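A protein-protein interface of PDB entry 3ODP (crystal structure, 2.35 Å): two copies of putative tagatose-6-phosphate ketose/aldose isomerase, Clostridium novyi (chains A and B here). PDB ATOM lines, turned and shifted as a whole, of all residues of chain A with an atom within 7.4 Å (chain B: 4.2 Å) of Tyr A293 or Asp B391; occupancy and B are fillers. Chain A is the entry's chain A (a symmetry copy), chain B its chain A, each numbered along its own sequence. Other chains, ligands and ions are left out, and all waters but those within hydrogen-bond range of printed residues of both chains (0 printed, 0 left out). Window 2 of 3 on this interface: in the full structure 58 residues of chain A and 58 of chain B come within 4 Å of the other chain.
The backbone carbonyl oxygen of Val B97 sits at hydrogen-bond distance from the side-chain hydroxyl of Tyr A293 (3.1 Å).
The side-chain hydroxyl of Tyr A297 lies within hydrogen-bond range of the backbone NH of His B390, at 3.1 Å.
The side-chain carboxylate (OD1) of Asp A291 lies within hydrogen-bond range of the backbone NH (N) of Tyr A293 (3.0 Å).
OH of Tyr A293 sits at hydrogen-bond distance from OH of Tyr A297, at 2.8 Å.
The side-chain carboxylate (OD1) of Asp A291 is in hydrogen-bond range of the backbone NH (N) of Ala A294 (2.7 Å).
Tyr A293 touches Ser B98.
Tyr A293 touches Pro B100.
CE1 of Tyr A293 touches O of His B390 (3.7 Å).
Tyr A293 touches Asp B391 (CD1 to O, 3.8 Å).
Ser B98 touches Ala A294.
CG of Glu A296 touches ND1 of His B390 (3.2 Å).
Val B97 touches Tyr A297 (O to CE2, 3.5 Å).
Printed residues of chain B within 4 Å of Tyr A293: Val B97 (3.1 Å), Ser B98 (3.7 Å), Pro B100 (3.8 Å), His B390 (3.7 Å) and Asp B391 (3.8 Å).
Of the printed residues of chain B, Ala A294 touches Ser B98.
Of the printed residues of chain B, Glu A296 touches His B390.
Printed residues of chain B within 4 Å of Tyr A297: Val B97 (3.5 Å) and His B390 (3.1 Å).
Of the printed residues of chain A, Val B97 touches Tyr A293 (3.1 Å) and Tyr A297 (3.5 Å).
Of the printed residues of chain A, Ser B98 touches Tyr A293 (3.7 Å) and Ala A294 (3.2 Å).
Of chain A, only Tyr A293 (3.8 Å) comes within 4 Å of Asp B391.
The nearest residue of chain B that does not touch Tyr A293 is Tyr B392 (4.1 Å).
Hydrophobic or aromatic side chains of chain A within 4 Å of the printed part of chain B: Tyr A293, Ala A294 and Tyr A297.
Along chain A the printed residues that touch a printed residue of chain B span positions 293 to 297.
Of the 6 printed residues of chain B, 5 touch a printed residue of chain A.
Printed residues of chain B that touch a printed residue of chain A: Val B97, Ser B98, Pro B100, His B390 and Asp B391.
Hydrophobic or aromatic side chains of chain B that line the printed part of chain A: Val B97, Pro B100 and His B390.
Among the printed residues, 9 pairs touch across the chains.
Among the printed residues, no Asp or Glu carboxylate lies within 4 Å of a Lys or Arg side-chain nitrogen of the other chain.
No position is printed for both chains.
Of the 9 pairs that touch across the chains among the printed residues, none has its exchanged pair printed and touching as well.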
ATOM      1  N   SER A 289     -17.889  -3.213  11.949  1.00  0.00           N
ATOM      2  CA  SER A 289     -16.906  -3.122  10.875  1.00  0.00           C
ATOM      3  C   SER A 289     -17.578  -3.521   9.559  1.00  0.00           C
ATOM      4  O   SER A 289     -18.495  -4.345   9.554  1.00  0.00           O
ATOM      5  CB  SER A 289     -15.716  -4.057  11.142  1.00  0.00           C
ATOM      6  OG  SER A 289     -15.112  -3.826  12.407  1.00  0.00           O
ATOM      7  N   ASN A 290     -17.103  -2.943   8.454  1.00  0.00           N
ATOM      8  CA  ASN A 290     -17.493  -3.396   7.120  1.00  0.00           C
ATOM      9  C   ASN A 290     -16.532  -4.477   6.628  1.00  0.00           C
ATOM     10  O   ASN A 290     -16.864  -5.255   5.736  1.00  0.00           O
ATOM     11  CB  ASN A 290     -17.530  -2.233   6.110  1.00  0.00           C
ATOM     12  CG  ASN A 290     -18.840  -1.455   6.135  1.00  0.00           C
ATOM     13  OD1 ASN A 290     -19.751  -1.735   6.938  1.00  0.00           O
ATOM     14  ND2 ASN A 290     -18.943  -0.471   5.241  1.00  0.00           N
ATOM     15  N   ASP A 291     -15.333  -4.523   7.194  1.00  0.00           N
ATOM     16  CA  ASP A 291     -14.424  -5.602   6.855  1.00  0.00           C
ATOM     17  C   ASP A 291     -15.150  -6.895   7.176  1.00  0.00           C
ATOM     18  O   ASP A 291     -15.527  -7.134   8.322  1.00  0.00           O
ATOM     19  CB  ASP A 291     -13.108  -5.524   7.621  1.00  0.00           C
ATOM     20  CG  ASP A 291     -12.225  -6.721   7.349  1.00  0.00           C
ATOM     21  OD1 ASP A 291     -12.484  -7.792   7.928  1.00  0.00           O
ATOM     22  OD2 ASP A 291     -11.285  -6.612   6.542  1.00  0.00           O
ATOM     23  N   THR A 292     -15.364  -7.712   6.152  1.00  0.00           N
ATOM     24  CA  THR A 292     -16.227  -8.885   6.287  1.00  0.00           C
ATOM     25  C   THR A 292     -15.672  -9.852   7.336  1.00  0.00           C
ATOM     26  O   THR A 292     -16.420 -10.393   8.144  1.00  0.00           O
ATOM     27  CB  THR A 292     -16.486  -9.587   4.927  1.00  0.00           C
ATOM     28  OG1 THR A 292     -17.096 -10.855   5.163  1.00  0.00           O
ATOM     29  CG2 THR A 292     -15.208  -9.800   4.138  1.00  0.00           C
ATOM     30  N   TYR A 293     -14.356 -10.028   7.363  1.00  0.00           N
ATOM     31  CA  TYR A 293     -13.754 -10.934   8.338  1.00  0.00           C
ATOM     32  C   TYR A 293     -13.899 -10.423   9.778  1.00  0.00           C
ATOM     33  O   TYR A 293     -14.295 -11.181  10.668  1.00  0.00           O
ATOM     34  CB  TYR A 293     -12.287 -11.206   8.001  1.00  0.00           C
ATOM     35  CG  TYR A 293     -11.567 -11.978   9.075  1.00  0.00           C
ATOM     36  CD1 TYR A 293     -11.761 -13.349   9.230  1.00  0.00           C
ATOM     37  CD2 TYR A 293     -10.693 -11.338   9.940  1.00  0.00           C
ATOM     38  CE1 TYR A 293     -11.095 -14.055  10.223  1.00  0.00           C
ATOM     39  CE2 TYR A 293     -10.033 -12.027  10.921  1.00  0.00           C
ATOM     40  CZ  TYR A 293     -10.234 -13.386  11.061  1.00  0.00           C
ATOM     41  OH  TYR A 293      -9.558 -14.055  12.050  1.00  0.00           O
ATOM     42  N   ALA A 294     -13.605  -9.142  10.000  1.00  0.00           N
ATOM     43  CA  ALA A 294     -13.665  -8.565  11.344  1.00  0.00           C
ATOM     44  C   ALA A 294     -15.090  -8.504  11.859  1.00  0.00           C
ATOM     45  O   ALA A 294     -15.322  -8.632  13.064  1.00  0.00           O
ATOM     46  CB  ALA A 294     -13.037  -7.179  11.368  1.00  0.00           C
ATOM     47  N   ARG A 295     -16.035  -8.323  10.938  1.00  0.00           N
ATOM     48  CA  ARG A 295     -17.455  -8.198  11.275  1.00  0.00           C
ATOM     49  C   ARG A 295     -18.004  -9.458  11.949  1.00  0.00           C
ATOM     50  O   ARG A 295     -18.861  -9.377  12.838  1.00  0.00           O
ATOM     51  CB  ARG A 295     -18.270  -7.892  10.020  1.00  0.00           C
ATOM     52  CG  ARG A 295     -19.683  -7.439  10.313  1.00  0.00           C
ATOM     53  CD  ARG A 295     -20.509  -7.301   9.046  1.00  0.00           C
ATOM     54  NE  ARG A 295     -21.796  -6.671   9.337  1.00  0.00           N
ATOM     55  CZ  ARG A 295     -22.011  -5.357   9.410  1.00  0.00           C
ATOM     56  NH1 ARG A 295     -21.043  -4.482   9.194  1.00  0.00           N
ATOM     57  NH2 ARG A 295     -23.221  -4.910   9.693  1.00  0.00           N
ATOM     58  N   GLU A 296     -17.509 -10.616  11.517  1.00  0.00           N
ATOM     59  CA  GLU A 296     -17.997 -11.898  12.000  1.00  0.00           C
ATOM     60  C   GLU A 296     -17.945 -11.935  13.531  1.00  0.00           C
ATOM     61  O   GLU A 296     -18.906 -12.328  14.188  1.00  0.00           O
ATOM     62  CB  GLU A 296     -17.183 -13.050  11.384  1.00  0.00           C
ATOM     63  CG  GLU A 296     -18.040 -14.224  10.893  1.00  0.00           C
ATOM     64  CD  GLU A 296     -18.734 -13.952   9.580  1.00  0.00           C
ATOM     65  OE1 GLU A 296     -18.035 -13.900   8.548  1.00  0.00           O
ATOM     66  OE2 GLU A 296     -19.975 -13.810   9.575  1.00  0.00           O
ATOM     67  N   TYR A 297     -16.830 -11.478  14.088  1.00  0.00           N
ATOM     68  CA  TYR A 297     -16.634 -11.434  15.539  1.00  0.00           C
ATOM     69  C   TYR A 297     -17.637 -10.541  16.260  1.00  0.00           C
ATOM     70  O   TYR A 297     -17.997 -10.820  17.411  1.00  0.00           O
ATOM     71  CB  TYR A 297     -15.221 -10.971  15.852  1.00  0.00           C
ATOM     72  CG  TYR A 297     -14.205 -11.949  15.344  1.00  0.00           C
ATOM     73  CD1 TYR A 297     -13.970 -13.140  16.024  1.00  0.00           C
ATOM     74  CD2 TYR A 297     -13.508 -11.712  14.162  1.00  0.00           C
ATOM     75  CE1 TYR A 297     -13.058 -14.048  15.560  1.00  0.00           C
ATOM     76  CE2 TYR A 297     -12.588 -12.625  13.685  1.00  0.00           C
ATOM     77  CZ  TYR A 297     -12.368 -13.792  14.395  1.00  0.00           C
ATOM     78  OH  TYR A 297     -11.460 -14.717  13.944  1.00  0.00           O
ATOM     79  N   GLU A 298     -18.083  -9.483  15.581  1.00  0.00           N
ATOM     80  CA  GLU A 298     -19.027  -8.532  16.156  1.00  0.00           C
ATOM     81  C   GLU A 298     -20.450  -9.102  16.179  1.00  0.00           C
ATOM     82  O   GLU A 298     -21.231  -8.776  17.076  1.00  0.00           O
ATOM     83  CB  GLU A 298     -18.979  -7.207  15.388  1.00  0.00           C
ATOM     84  CG  GLU A 298     -17.620  -6.493  15.518  1.00  0.00           C
ATOM     85  CD  GLU A 298     -17.206  -5.715  14.270  1.00  0.00           C
ATOM     86  OE1 GLU A 298     -18.048  -5.465  13.396  1.00  0.00           O
ATOM     87  OE2 GLU A 298     -16.028  -5.349  14.155  1.00  0.00           O
ATOM     88  N   VAL B  97      -6.669 -10.625  16.385  1.00  0.00           N
ATOM     89  CA  VAL B  97      -7.620 -11.620  15.859  1.00  0.00           C
ATOM     90  C   VAL B  97      -8.750 -11.036  15.020  1.00  0.00           C
ATOM     91  O   VAL B  97      -9.247 -11.696  14.099  1.00  0.00           O
ATOM     92  CB  VAL B  97      -8.215 -12.498  17.003  1.00  0.00           C
ATOM     93  CG1 VAL B  97      -9.406 -13.313  16.511  1.00  0.00           C
ATOM     94  CG2 VAL B  97      -7.140 -13.414  17.576  1.00  0.00           C
ATOM     95  N   SER B  98      -9.188  -9.823  15.331  1.00  0.00           N
ATOM     96  CA  SER B  98     -10.222  -9.197  14.506  1.00  0.00           C
ATOM     97  C   SER B  98      -9.617  -8.525  13.266  1.00  0.00           C
ATOM     98  O   SER B  98     -10.262  -8.482  12.224  1.00  0.00           O
ATOM     99  CB  SER B  98     -11.104  -8.225  15.313  1.00  0.00           C
ATOM    100  OG  SER B  98     -10.366  -7.214  15.970  1.00  0.00           O
ATOM    101  N   PRO B 100      -5.979  -8.854  11.720  1.00  0.00           N
ATOM    102  CA  PRO B 100      -4.577  -9.253  11.634  1.00  0.00           C
ATOM    103  C   PRO B 100      -3.774  -8.400  10.659  1.00  0.00           C
ATOM    104  O   PRO B 100      -2.587  -8.173  10.886  1.00  0.00           O
ATOM    105  CB  PRO B 100      -4.663 -10.699  11.130  1.00  0.00           C
ATOM    106  CG  PRO B 100      -5.968 -10.778  10.467  1.00  0.00           C
ATOM    107  CD  PRO B 100      -6.868  -9.936  11.278  1.00  0.00           C
ATOM    108  N   HIS B 390     -12.914 -17.431  13.453  1.00  0.00           N
ATOM    109  CA  HIS B 390     -13.500 -17.517  12.097  1.00  0.00           C
ATOM    110  C   HIS B 390     -12.471 -17.744  10.990  1.00  0.00           C
ATOM    111  O   HIS B 390     -11.274 -17.578  11.193  1.00  0.00           O
ATOM    112  CB  HIS B 390     -14.345 -16.271  11.794  1.00  0.00           C
ATOM    113  CG  HIS B 390     -15.651 -16.236  12.526  1.00  0.00           C
ATOM    114  ND1 HIS B 390     -16.776 -16.891  12.074  1.00  0.00           N
ATOM    115  CD2 HIS B 390     -16.011 -15.623  13.678  1.00  0.00           C
ATOM    116  CE1 HIS B 390     -17.771 -16.685  12.918  1.00  0.00           C
ATOM    117  NE2 HIS B 390     -17.334 -15.916  13.899  1.00  0.00           N
ATOM    118  N   ASP B 391     -12.965 -18.100   9.810  1.00  0.00           N
ATOM    119  CA  ASP B 391     -12.121 -18.674   8.767  1.00  0.00           C
ATOM    120  C   ASP B 391     -11.300 -17.629   8.004  1.00  0.00           C
ATOM    121  O   ASP B 391     -11.838 -16.672   7.409  1.00  0.00           O
ATOM    122  CB  ASP B 391     -12.946 -19.542   7.797  1.00  0.00           C
ATOM    123  CG  ASP B 391     -12.412 -20.967   7.701  1.00  0.00           C
ATOM    124  OD1 ASP B 391     -11.338 -21.252   8.285  1.00  0.00           O
ATOM    125  OD2 ASP B 391     -13.076 -21.805   7.058  1.00  0.00           O
ATOM    126  N   TYR B 392      -9.990 -17.887   8.003  1.00  0.00           N
ATOM    127  CA  TYR B 392      -8.939 -16.962   7.557  1.00  0.00           C
ATOM    128  C   TYR B 392      -9.046 -16.556   6.085  1.00  0.00           C
ATOM    129  O   TYR B 392      -8.079 -16.054   5.501  1.00  0.00           O
ATOM    130  CB  TYR B 392      -7.558 -17.603   7.803  1.00  0.00           C
ATOM    131  CG  TYR B 392      -7.331 -18.107   9.222  1.00  0.00           C
ATOM    132  CD1 TYR B 392      -7.806 -17.390  10.320  1.00  0.00           C
ATOM    133  CD2 TYR B 392      -6.623 -19.291   9.464  1.00  0.00           C
ATOM    134  CE1 TYR B 392      -7.599 -17.834  11.616  1.00  0.00           C
ATOM    135  CE2 TYR B 392      -6.406 -19.742  10.765  1.00  0.00           C
ATOM    136  CZ  TYR B 392      -6.895 -18.999  11.837  1.00  0.00           C
ATOM    137  OH  TYR B 392      -6.705 -19.406  13.134  1.00  0.00           O
